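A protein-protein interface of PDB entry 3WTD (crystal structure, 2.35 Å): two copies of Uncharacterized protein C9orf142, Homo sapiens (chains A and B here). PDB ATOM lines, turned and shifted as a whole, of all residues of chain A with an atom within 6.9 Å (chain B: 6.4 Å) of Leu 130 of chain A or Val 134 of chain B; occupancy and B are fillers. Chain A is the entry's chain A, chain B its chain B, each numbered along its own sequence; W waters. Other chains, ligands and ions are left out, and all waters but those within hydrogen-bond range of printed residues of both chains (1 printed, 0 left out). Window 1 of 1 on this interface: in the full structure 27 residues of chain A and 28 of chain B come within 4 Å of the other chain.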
ATOM      1  N   SER A   7      31.263  -0.699  -1.896  1.00  0.00           N
ATOM      2  CA  SER A   7      30.836   0.162  -2.998  1.00  0.00           C
ATOM      3  C   SER A   7      30.682  -0.662  -4.274  1.00  0.00           C
ATOM      4  O   SER A   7      31.664  -1.200  -4.778  1.00  0.00           O
ATOM      5  CB  SER A   7      31.837   1.301  -3.206  1.00  0.00           C
ATOM      6  OG  SER A   7      31.192   2.465  -3.691  1.00  0.00           O
ATOM      7  N   PRO A   8      29.448  -0.744  -4.812  1.00  0.00           N
ATOM      8  CA  PRO A   8      29.066  -1.719  -5.852  1.00  0.00           C
ATOM      9  C   PRO A   8      29.835  -1.536  -7.158  1.00  0.00           C
ATOM     10  O   PRO A   8      29.749  -0.480  -7.776  1.00  0.00           O
ATOM     11  CB  PRO A   8      27.568  -1.446  -6.074  1.00  0.00           C
ATOM     12  CG  PRO A   8      27.167  -0.438  -5.021  1.00  0.00           C
ATOM     13  CD  PRO A   8      28.408   0.277  -4.613  1.00  0.00           C
ATOM     14  N   LEU A  10      31.069  -1.527 -11.029  1.00  0.00           N
ATOM     15  CA  LEU A  10      30.454  -1.408 -12.342  1.00  0.00           C
ATOM     16  C   LEU A  10      31.480  -0.899 -13.344  1.00  0.00           C
ATOM     17  O   LEU A  10      32.516  -0.354 -12.967  1.00  0.00           O
ATOM     18  CB  LEU A  10      29.238  -0.477 -12.306  1.00  0.00           C
ATOM     19  CG  LEU A  10      29.399   1.022 -12.015  1.00  0.00           C
ATOM     20  CD1 LEU A  10      29.774   1.813 -13.254  1.00  0.00           C
ATOM     21  CD2 LEU A  10      28.114   1.564 -11.441  1.00  0.00           C
ATOM     22  N   VAL A  23      26.235  -0.705 -19.528  1.00  0.00           N
ATOM     23  CA  VAL A  23      26.797  -0.783 -18.183  1.00  0.00           C
ATOM     24  C   VAL A  23      26.687  -2.215 -17.666  1.00  0.00           C
ATOM     25  O   VAL A  23      25.690  -2.911 -17.876  1.00  0.00           O
ATOM     26  CB  VAL A  23      26.128   0.220 -17.203  1.00  0.00           C
ATOM     27  CG1 VAL A  23      24.638   0.227 -17.354  1.00  0.00           C
ATOM     28  CG2 VAL A  23      26.518  -0.064 -15.761  1.00  0.00           C
ATOM     29  N   ALA A 125      15.575   1.855 -10.474  1.00  0.00           N
ATOM     30  CA  ALA A 125      16.414   1.964  -9.280  1.00  0.00           C
ATOM     31  C   ALA A 125      17.884   2.154  -9.649  1.00  0.00           C
ATOM     32  O   ALA A 125      18.623   2.827  -8.944  1.00  0.00           O
ATOM     33  CB  ALA A 125      16.255   0.733  -8.388  1.00  0.00           C
ATOM     34  N   LEU A 126      18.300   1.545 -10.751  1.00  0.00           N
ATOM     35  CA  LEU A 126      19.657   1.706 -11.251  1.00  0.00           C
ATOM     36  C   LEU A 126      19.936   3.184 -11.533  1.00  0.00           C
ATOM     37  O   LEU A 126      20.896   3.749 -11.043  1.00  0.00           O
ATOM     38  CB  LEU A 126      19.868   0.883 -12.518  1.00  0.00           C
ATOM     39  CG  LEU A 126      21.250   1.074 -13.136  1.00  0.00           C
ATOM     40  CD1 LEU A 126      22.299   0.498 -12.221  1.00  0.00           C
ATOM     41  CD2 LEU A 126      21.350   0.460 -14.515  1.00  0.00           C
ATOM     42  N   THR A 127      19.065   3.806 -12.312  1.00  0.00           N
ATOM     43  CA  THR A 127      19.219   5.212 -12.653  1.00  0.00           C
ATOM     44  C   THR A 127      19.227   6.110 -11.426  1.00  0.00           C
ATOM     45  O   THR A 127      20.103   6.957 -11.289  1.00  0.00           O
ATOM     46  CB  THR A 127      18.108   5.662 -13.616  1.00  0.00           C
ATOM     47  OG1 THR A 127      18.244   4.912 -14.819  1.00  0.00           O
ATOM     48  CG2 THR A 127      18.243   7.157 -13.946  1.00  0.00           C
ATOM     49  N   LEU A 128      18.283   5.903 -10.516  1.00  0.00           N
ATOM     50  CA  LEU A 128      18.168   6.786  -9.370  1.00  0.00           C
ATOM     51  C   LEU A 128      19.357   6.602  -8.423  1.00  0.00           C
ATOM     52  O   LEU A 128      19.851   7.568  -7.838  1.00  0.00           O
ATOM     53  CB  LEU A 128      16.843   6.552  -8.639  1.00  0.00           C
ATOM     54  CG  LEU A 128      15.575   6.874  -9.447  1.00  0.00           C
ATOM     55  CD1 LEU A 128      14.327   6.338  -8.743  1.00  0.00           C
ATOM     56  CD2 LEU A 128      15.433   8.378  -9.710  1.00  0.00           C
ATOM     57  N   GLY A 129      19.814   5.361  -8.281  1.00  0.00           N
ATOM     58  CA  GLY A 129      20.940   5.056  -7.414  1.00  0.00           C
ATOM     59  C   GLY A 129      22.258   5.597  -7.953  1.00  0.00           C
ATOM     60  O   GLY A 129      23.081   6.091  -7.200  1.00  0.00           O
ATOM     61  N   LEU A 130      22.461   5.502  -9.262  1.00  0.00           N
ATOM     62  CA  LEU A 130      23.627   6.110  -9.895  1.00  0.00           C
ATOM     63  C   LEU A 130      23.704   7.610  -9.635  1.00  0.00           C
ATOM     64  O   LEU A 130      24.769   8.142  -9.347  1.00  0.00           O
ATOM     65  CB  LEU A 130      23.598   5.875 -11.391  1.00  0.00           C
ATOM     66  CG  LEU A 130      23.836   4.454 -11.879  1.00  0.00           C
ATOM     67  CD1 LEU A 130      23.691   4.441 -13.380  1.00  0.00           C
ATOM     68  CD2 LEU A 130      25.211   3.987 -11.437  1.00  0.00           C
ATOM     69  N   ALA A 131      22.564   8.284  -9.762  1.00  0.00           N
ATOM     70  CA  ALA A 131      22.513   9.715  -9.595  1.00  0.00           C
ATOM     71  C   ALA A 131      22.896  10.083  -8.172  1.00  0.00           C
ATOM     72  O   ALA A 131      23.604  11.055  -7.947  1.00  0.00           O
ATOM     73  CB  ALA A 131      21.150  10.232  -9.931  1.00  0.00           C
ATOM     74  N   LYS A 132      22.426   9.290  -7.218  1.00  0.00           N
ATOM     75  CA  LYS A 132      22.717   9.542  -5.824  1.00  0.00           C
ATOM     76  C   LYS A 132      24.201   9.295  -5.498  1.00  0.00           C
ATOM     77  O   LYS A 132      24.795  10.004  -4.684  1.00  0.00           O
ATOM     78  CB  LYS A 132      21.834   8.678  -4.932  1.00  0.00           C
ATOM     79  CG  LYS A 132      22.207   8.805  -3.453  1.00  0.00           C
ATOM     80  CD  LYS A 132      21.165   8.203  -2.540  1.00  0.00           C
ATOM     81  CE  LYS A 132      21.306   8.758  -1.131  1.00  0.00           C
ATOM     82  NZ  LYS A 132      19.978   8.793  -0.464  1.00  0.00           N
ATOM     83  N   ARG A 133      24.787   8.292  -6.139  1.00  0.00           N
ATOM     84  CA  ARG A 133      26.211   8.016  -6.000  1.00  0.00           C
ATOM     85  C   ARG A 133      27.068   9.150  -6.534  1.00  0.00           C
ATOM     86  O   ARG A 133      28.001   9.598  -5.868  1.00  0.00           O
ATOM     87  CB  ARG A 133      26.581   6.722  -6.724  1.00  0.00           C
ATOM     88  CG  ARG A 133      26.440   5.488  -5.860  1.00  0.00           C
ATOM     89  CD  ARG A 133      26.698   4.229  -6.666  1.00  0.00           C
ATOM     90  NE  ARG A 133      28.106   3.848  -6.677  1.00  0.00           N
ATOM     91  CZ  ARG A 133      28.565   2.735  -7.242  1.00  0.00           C
ATOM     92  NH1 ARG A 133      27.727   1.903  -7.855  1.00  0.00           N
ATOM     93  NH2 ARG A 133      29.861   2.455  -7.200  1.00  0.00           N
ATOM     94  N   VAL A 134      26.766   9.585  -7.752  1.00  0.00           N
ATOM     95  CA  VAL A 134      27.462  10.722  -8.344  1.00  0.00           C
ATOM     96  C   VAL A 134      27.460  11.909  -7.390  1.00  0.00           C
ATOM     97  O   VAL A 134      28.521  12.466  -7.092  1.00  0.00           O
ATOM     98  CB  VAL A 134      26.834  11.139  -9.675  1.00  0.00           C
ATOM     99  CG1 VAL A 134      27.324  12.517 -10.094  1.00  0.00           C
ATOM    100  CG2 VAL A 134      27.141  10.090 -10.753  1.00  0.00           C
ATOM    101  N   TRP A 135      26.274  12.282  -6.900  1.00  0.00           N
ATOM    102  CA  TRP A 135      26.148  13.406  -5.971  1.00  0.00           C
ATOM    103  C   TRP A 135      27.030  13.192  -4.740  1.00  0.00           C
ATOM    104  O   TRP A 135      27.637  14.129  -4.231  1.00  0.00           O
ATOM    105  CB  TRP A 135      24.687  13.612  -5.543  1.00  0.00           C
ATOM    106  CG  TRP A 135      24.505  14.797  -4.609  1.00  0.00           C
ATOM    107  CD1 TRP A 135      24.204  16.086  -4.963  1.00  0.00           C
ATOM    108  CD2 TRP A 135      24.606  14.793  -3.178  1.00  0.00           C
ATOM    109  NE1 TRP A 135      24.109  16.875  -3.846  1.00  0.00           N
ATOM    110  CE2 TRP A 135      24.353  16.105  -2.731  1.00  0.00           C
ATOM    111  CE3 TRP A 135      24.885  13.804  -2.220  1.00  0.00           C
ATOM    112  CZ2 TRP A 135      24.381  16.462  -1.385  1.00  0.00           C
ATOM    113  CZ3 TRP A 135      24.906  14.157  -0.880  1.00  0.00           C
ATOM    114  CH2 TRP A 135      24.656  15.472  -0.477  1.00  0.00           C
ATOM    115  N   SER A 136      27.112  11.949  -4.276  1.00  0.00           N
ATOM    116  CA  SER A 136      27.860  11.641  -3.060  1.00  0.00           C
ATOM    117  C   SER A 136      29.368  11.657  -3.301  1.00  0.00           C
ATOM    118  O   SER A 136      30.140  12.211  -2.509  1.00  0.00           O
ATOM    119  CB  SER A 136      27.432  10.287  -2.511  1.00  0.00           C
ATOM    120  OG  SER A 136      27.838  10.158  -1.161  1.00  0.00           O
ATOM    121  N   LEU A 137      29.774  11.053  -4.411  1.00  0.00           N
ATOM    122  CA  LEU A 137      31.180  10.985  -4.782  1.00  0.00           C
ATOM    123  C   LEU A 137      31.757  12.368  -5.083  1.00  0.00           C
ATOM    124  O   LEU A 137      32.910  12.642  -4.776  1.00  0.00           O
ATOM    125  CB  LEU A 137      31.367  10.076  -5.997  1.00  0.00           C
ATOM    126  CG  LEU A 137      31.059   8.587  -5.822  1.00  0.00           C
ATOM    127  CD1 LEU A 137      30.923   7.876  -7.191  1.00  0.00           C
ATOM    128  CD2 LEU A 137      32.133   7.939  -4.983  1.00  0.00           C
ATOM    129  N   LEU B  10      23.810  18.016 -10.247  1.00  0.00           N
ATOM    130  CA  LEU B  10      22.577  17.279 -10.045  1.00  0.00           C
ATOM    131  C   LEU B  10      22.353  17.068  -8.572  1.00  0.00           C
ATOM    132  O   LEU B  10      23.228  17.328  -7.751  1.00  0.00           O
ATOM    133  CB  LEU B  10      22.591  15.940 -10.778  1.00  0.00           C
ATOM    134  CG  LEU B  10      23.625  14.837 -10.494  1.00  0.00           C
ATOM    135  CD1 LEU B  10      23.381  14.098  -9.198  1.00  0.00           C
ATOM    136  CD2 LEU B  10      23.582  13.854 -11.622  1.00  0.00           C
ATOM    137  N   THR B  12      19.510  14.442  -5.938  1.00  0.00           N
ATOM    138  CA  THR B  12      18.408  13.504  -5.867  1.00  0.00           C
ATOM    139  C   THR B  12      17.474  13.892  -4.740  1.00  0.00           C
ATOM    140  O   THR B  12      17.875  14.536  -3.781  1.00  0.00           O
ATOM    141  CB  THR B  12      18.877  12.058  -5.647  1.00  0.00           C
ATOM    142  OG1 THR B  12      19.600  11.968  -4.413  1.00  0.00           O
ATOM    143  CG2 THR B  12      19.743  11.605  -6.795  1.00  0.00           C
ATOM    144  N   LEU B 126      21.139   9.531 -20.037  1.00  0.00           N
ATOM    145  CA  LEU B 126      21.348   9.907 -18.633  1.00  0.00           C
ATOM    146  C   LEU B 126      21.898   8.734 -17.795  1.00  0.00           C
ATOM    147  O   LEU B 126      22.912   8.867 -17.099  1.00  0.00           O
ATOM    148  CB  LEU B 126      20.039  10.423 -18.008  1.00  0.00           C
ATOM    149  CG  LEU B 126      20.148  10.828 -16.527  1.00  0.00           C
ATOM    150  CD1 LEU B 126      20.941  12.119 -16.410  1.00  0.00           C
ATOM    151  CD2 LEU B 126      18.786  10.924 -15.769  1.00  0.00           C
ATOM    152  N   THR B 127      21.246   7.585 -17.892  1.00  0.00           N
ATOM    153  CA  THR B 127      21.684   6.386 -17.181  1.00  0.00           C
ATOM    154  C   THR B 127      23.122   5.996 -17.546  1.00  0.00           C
ATOM    155  O   THR B 127      23.977   5.769 -16.682  1.00  0.00           O
ATOM    156  CB  THR B 127      20.741   5.211 -17.488  1.00  0.00           C
ATOM    157  OG1 THR B 127      19.402   5.577 -17.141  1.00  0.00           O
ATOM    158  CG2 THR B 127      21.138   3.960 -16.711  1.00  0.00           C
ATOM    159  N   LEU B 128      23.392   5.933 -18.839  1.00  0.00           N
ATOM    160  CA  LEU B 128      24.712   5.521 -19.296  1.00  0.00           C
ATOM    161  C   LEU B 128      25.773   6.558 -18.892  1.00  0.00           C
ATOM    162  O   LEU B 128      26.847   6.196 -18.427  1.00  0.00           O
ATOM    163  CB  LEU B 128      24.698   5.301 -20.809  1.00  0.00           C
ATOM    164  CG  LEU B 128      23.857   4.098 -21.258  1.00  0.00           C
ATOM    165  CD1 LEU B 128      23.546   4.160 -22.745  1.00  0.00           C
ATOM    166  CD2 LEU B 128      24.572   2.787 -20.947  1.00  0.00           C
ATOM    167  N   GLY B 129      25.445   7.841 -19.042  1.00  0.00           N
ATOM    168  CA  GLY B 129      26.338   8.920 -18.651  1.00  0.00           C
ATOM    169  C   GLY B 129      26.666   8.945 -17.166  1.00  0.00           C
ATOM    170  O   GLY B 129      27.800   9.236 -16.781  1.00  0.00           O
ATOM    171  N   LEU B 130      25.674   8.660 -16.327  1.00  0.00           N
ATOM    172  CA  LEU B 130      25.880   8.626 -14.877  1.00  0.00           C
ATOM    173  C   LEU B 130      26.837   7.505 -14.503  1.00  0.00           C
ATOM    174  O   LEU B 130      27.715   7.684 -13.665  1.00  0.00           O
ATOM    175  CB  LEU B 130      24.560   8.432 -14.127  1.00  0.00           C
ATOM    176  CG  LEU B 130      23.568   9.600 -14.190  1.00  0.00           C
ATOM    177  CD1 LEU B 130      22.212   9.234 -13.547  1.00  0.00           C
ATOM    178  CD2 LEU B 130      24.143  10.856 -13.572  1.00  0.00           C
ATOM    179  N   ALA B 131      26.658   6.350 -15.134  1.00  0.00           N
ATOM    180  CA  ALA B 131      27.479   5.182 -14.847  1.00  0.00           C
ATOM    181  C   ALA B 131      28.921   5.430 -15.230  1.00  0.00           C
ATOM    182  O   ALA B 131      29.829   5.042 -14.502  1.00  0.00           O
ATOM    183  CB  ALA B 131      26.951   3.960 -15.567  1.00  0.00           C
ATOM    184  N   LYS B 132      29.125   6.070 -16.373  1.00  0.00           N
ATOM    185  CA  LYS B 132      30.452   6.522 -16.751  1.00  0.00           C
ATOM    186  C   LYS B 132      31.032   7.466 -15.679  1.00  0.00           C
ATOM    187  O   LYS B 132      32.181   7.297 -15.275  1.00  0.00           O
ATOM    188  CB  LYS B 132      30.409   7.211 -18.118  1.00  0.00           C
ATOM    189  CG  LYS B 132      31.769   7.592 -18.699  1.00  0.00           C
ATOM    190  CD  LYS B 132      32.424   6.424 -19.408  1.00  0.00           C
ATOM    191  CE  LYS B 132      33.615   6.886 -20.234  1.00  0.00           C
ATOM    192  NZ  LYS B 132      34.159   5.794 -21.089  1.00  0.00           N
ATOM    193  N   ARG B 133      30.238   8.440 -15.221  1.00  0.00           N
ATOM    194  CA  ARG B 133      30.667   9.386 -14.164  1.00  0.00           C
ATOM    195  C   ARG B 133      31.063   8.689 -12.867  1.00  0.00           C
ATOM    196  O   ARG B 133      32.121   8.966 -12.300  1.00  0.00           O
ATOM    197  CB  ARG B 133      29.564  10.387 -13.834  1.00  0.00           C
ATOM    198  CG  ARG B 133      29.572  11.641 -14.643  1.00  0.00           C
ATOM    199  CD  ARG B 133      29.366  12.830 -13.731  1.00  0.00           C
ATOM    200  NE  ARG B 133      28.078  13.455 -13.965  1.00  0.00           N
ATOM    201  CZ  ARG B 133      27.653  14.534 -13.325  1.00  0.00           C
ATOM    202  NH1 ARG B 133      28.423  15.098 -12.414  1.00  0.00           N
ATOM    203  NH2 ARG B 133      26.461  15.047 -13.598  1.00  0.00           N
ATOM    204  N   VAL B 134      30.182   7.814 -12.388  1.00  0.00           N
ATOM    205  CA  VAL B 134      30.438   7.050 -11.179  1.00  0.00           C
ATOM    206  C   VAL B 134      31.777   6.335 -11.287  1.00  0.00           C
ATOM    207  O   VAL B 134      32.631   6.457 -10.402  1.00  0.00           O
ATOM    208  CB  VAL B 134      29.335   6.016 -10.911  1.00  0.00           C
ATOM    209  CG1 VAL B 134      29.758   5.056  -9.781  1.00  0.00           C
ATOM    210  CG2 VAL B 134      28.025   6.716 -10.579  1.00  0.00           C
ATOM    211  N   TRP B 135      31.964   5.618 -12.391  1.00  0.00           N
ATOM    212  CA  TRP B 135      33.194   4.873 -12.618  1.00  0.00           C
ATOM    213  C   TRP B 135      34.393   5.814 -12.618  1.00  0.00           C
ATOM    214  O   TRP B 135      35.421   5.521 -12.015  1.00  0.00           O
ATOM    215  CB  TRP B 135      33.123   4.084 -13.934  1.00  0.00           C
ATOM    216  CG  TRP B 135      34.367   3.266 -14.234  1.00  0.00           C
ATOM    217  CD1 TRP B 135      34.583   1.949 -13.932  1.00  0.00           C
ATOM    218  CD2 TRP B 135      35.559   3.726 -14.896  1.00  0.00           C
ATOM    219  NE1 TRP B 135      35.832   1.561 -14.365  1.00  0.00           N
ATOM    220  CE2 TRP B 135      36.445   2.628 -14.962  1.00  0.00           C
ATOM    221  CE3 TRP B 135      35.951   4.952 -15.445  1.00  0.00           C
ATOM    222  CZ2 TRP B 135      37.708   2.729 -15.552  1.00  0.00           C
ATOM    223  CZ3 TRP B 135      37.201   5.045 -16.035  1.00  0.00           C
ATOM    224  CH2 TRP B 135      38.066   3.939 -16.082  1.00  0.00           C
ATOM    225  N   SER B 136      34.247   6.953 -13.283  1.00  0.00           N
ATOM    226  CA  SER B 136      35.319   7.933 -13.364  1.00  0.00           C
ATOM    227  C   SER B 136      35.593   8.584 -12.004  1.00  0.00           C
ATOM    228  O   SER B 136      36.747   8.779 -11.628  1.00  0.00           O
ATOM    229  CB  SER B 136      34.980   8.998 -14.407  1.00  0.00           C
ATOM    230  OG  SER B 136      35.895  10.079 -14.342  1.00  0.00           O
ATOM    231  N   LEU B 137      34.531   8.906 -11.271  1.00  0.00           N
ATOM    232  CA  LEU B 137      34.660   9.539  -9.958  1.00  0.00           C
ATOM    233  C   LEU B 137      35.346   8.640  -8.937  1.00  0.00           C
ATOM    234  O   LEU B 137      36.236   9.081  -8.211  1.00  0.00           O
ATOM    235  CB  LEU B 137      33.287   9.951  -9.424  1.00  0.00           C
ATOM    236  CG  LEU B 137      32.710  11.217 -10.049  1.00  0.00           C
ATOM    237  CD1 LEU B 137      31.229  11.335  -9.736  1.00  0.00           C
ATOM    238  CD2 LEU B 137      33.482  12.427  -9.538  1.00  0.00           C
ATOM    239  N   GLU B 138      34.925   7.383  -8.870  1.00  0.00           N
ATOM    240  CA  GLU B 138      35.476   6.472  -7.875  1.00  0.00           C
ATOM    241  C   GLU B 138      36.945   6.189  -8.155  1.00  0.00           C
ATOM    242  O   GLU B 138      37.725   5.916  -7.242  1.00  0.00           O
ATOM    243  CB  GLU B 138      34.670   5.180  -7.827  1.00  0.00           C
ATOM    244  CG  GLU B 138      33.769   5.102  -6.607  1.00  0.00           C
ATOM    245  CD  GLU B 138      32.554   4.234  -6.827  1.00  0.00           C
ATOM    246  OE1 GLU B 138      32.368   3.765  -7.968  1.00  0.00           O
ATOM    247  OE2 GLU B 138      31.783   4.025  -5.863  1.00  0.00           O
ATOM    248  N   ARG B 139      37.320   6.284  -9.425  1.00  0.00           N
ATOM    249  CA  ARG B 139      38.714   6.172  -9.819  1.00  0.00           C
ATOM    250  C   ARG B 139      39.500   7.390  -9.333  1.00  0.00           C
ATOM    251  O   ARG B 139      40.571   7.254  -8.740  1.00  0.00           O
ATOM    252  CB  ARG B 139      38.822   6.028 -11.335  1.00  0.00           C
ATOM    253  CG  ARG B 139      40.061   5.314 -11.801  1.00  0.00           C
ATOM    254  CD  ARG B 139      39.831   4.694 -13.160  1.00  0.00           C
ATOM    255  NE  ARG B 139      40.029   5.650 -14.244  1.00  0.00           N
ATOM    256  CZ  ARG B 139      41.074   5.629 -15.067  1.00  0.00           C
ATOM    257  NH1 ARG B 139      42.007   4.695 -14.930  1.00  0.00           N
ATOM    258  NH2 ARG B 139      41.180   6.536 -16.032  1.00  0.00           N
HETATM  259  O   HOH W   1      29.713   4.739  -4.594  1.00  0.00           O
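Printed residues of chain A that touch a printed residue of chain B: Ser 7, Leu 10, Thr 127, Leu 130, Ala 131, Lys 132, Arg 133, Val 134, Trp 135 and Leu 137.
Hydrophobic or aromatic side chains of chain A within 4 Å of the printed part of chain B: Leu 10, Leu 130, Ala 131, Val 134, Trp 135 and Leu 137.
Of the 16 printed residues of chain B, 10 touch a printed residue of chain A.
Along chain B the printed residues that touch a printed residue of chain A span positions 10 to 138.
Among the printed residues, 23 pairs touch across the chains.
Water W1 lies within hydrogen-bond range of OE2 of Glu 138 of chain B, NE of Arg 133 of chain A and OG of Ser 7 of chain A.
Leu 130 of chain A touches its own counterpart, Leu 130 of chain B.
Val 134 of chain A touches its own counterpart, Val 134 of chain B.
Val 134 of chain A touches Leu 137 of chain B, and with the chains exchanged Leu 137 of chain A touches Val 134 of chain B.
Leu 137 of chain A touches its own counterpart, Leu 137 of chain B.
Positions printed for both chains: 10, 126, 127, 128, 129, 130, 131, 132, 133, 134, 135, 136 and 137.
Of the 23 pairs that touch across the chains among the printed residues, 18 have their exchanged pair printed and touching as well.
The side-chain hydroxyl (OG1) of Thr 127 of chain A lies within hydrogen-bond range of the side-chain hydroxyl (OG1) of Thr 127 of chain B.
The side-chain carboxylate (OE2) of Glu 138 of chain B lies within hydrogen-bond range of the side-chain hydroxyl (OG) of Ser 7 of chain A, 2.7 Å away.
The guanidinium group of Arg 133 of chain A lies within salt-bridge range of the side-chain carboxylate of Glu 138 of chain B (2.8 Å).
Among the printed residues, merely in contact across the chains: Trp 135 of chain A with Leu 10 of chain B (3.2 Å), Leu 10 of chain A with Trp 135 of chain B (3.2 Å), Ala 131 of chain A with Leu 10 of chain B (3.3 Å), Leu 10 of chain A with Ala 131 of chain B (3.5 Å), Val 134 of chain A with Val 134 of chain B (3.5 Å), Lys 132 of chain A with Thr 12 of chain B (3.6 Å), Leu 130 of chain A with Thr 127 of chain B (3.6 Å), Val 134 of chain A with Arg 133 of chain B (3.6 Å), Arg 133 of chain A with Val 134 of chain B (3.6 Å), Leu 137 of chain A with Glu 138 of chain B (3.7 Å), Ala 131 of chain A with Thr 12 of chain B (3.7 Å), Leu 130 of chain A with Val 134 of chain B (3.8 Å), Val 134 of chain A with Leu 130 of chain B (3.8 Å), Thr 127 of chain A with Leu 130 of chain B (3.8 Å), Leu 137 of chain A with Leu 137 of chain B (3.9 Å), Leu 130 of chain A with Leu 130 of chain B (3.9 Å), Ala 131 of chain A with Leu 130 of chain B (3.9 Å), Leu 137 of chain A with Val 134 of chain B (3.9 Å), Leu 130 of chain A with Ala 131 of chain B (3.9 Å) and Val 134 of chain A with Leu 137 of chain B (3.95 Å).
O of Pro 8 of chain A sits at hydrogen-bond distance from NH2 of Arg 133 of chain A, at 3.0 Å.
Leu 130 of chain A touches four residues of chain B.
Of chain A, only Leu 130 (3.8 Å), Arg 133 (3.6 Å), Val 134 (3.5 Å) and Leu 137 (3.9 Å) come within 4 Å of Val 134 of chain B.
Of the printed residues of chain A, Leu 10 of chain B touches Ala 131 and Trp 135.
Printed residues of chain A within 4 Å of Trp 135 of chain B: Leu 10.
Printed residues of chain B within 4 Å of Ser 7 of chain A: Glu 138 (2.7 Å).
Printed residues of chain B within 4 Å of Lys 132 of chain A: Thr 12.
Ser 136 of chain B touches none of the printed residues of chain A.
Arg 139 of chain B touches none of the printed residues of chain A.
The nearest printed residue of chain A that does not touch Thr 127 of chain B is Leu 126 of chain A (4.1 Å).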
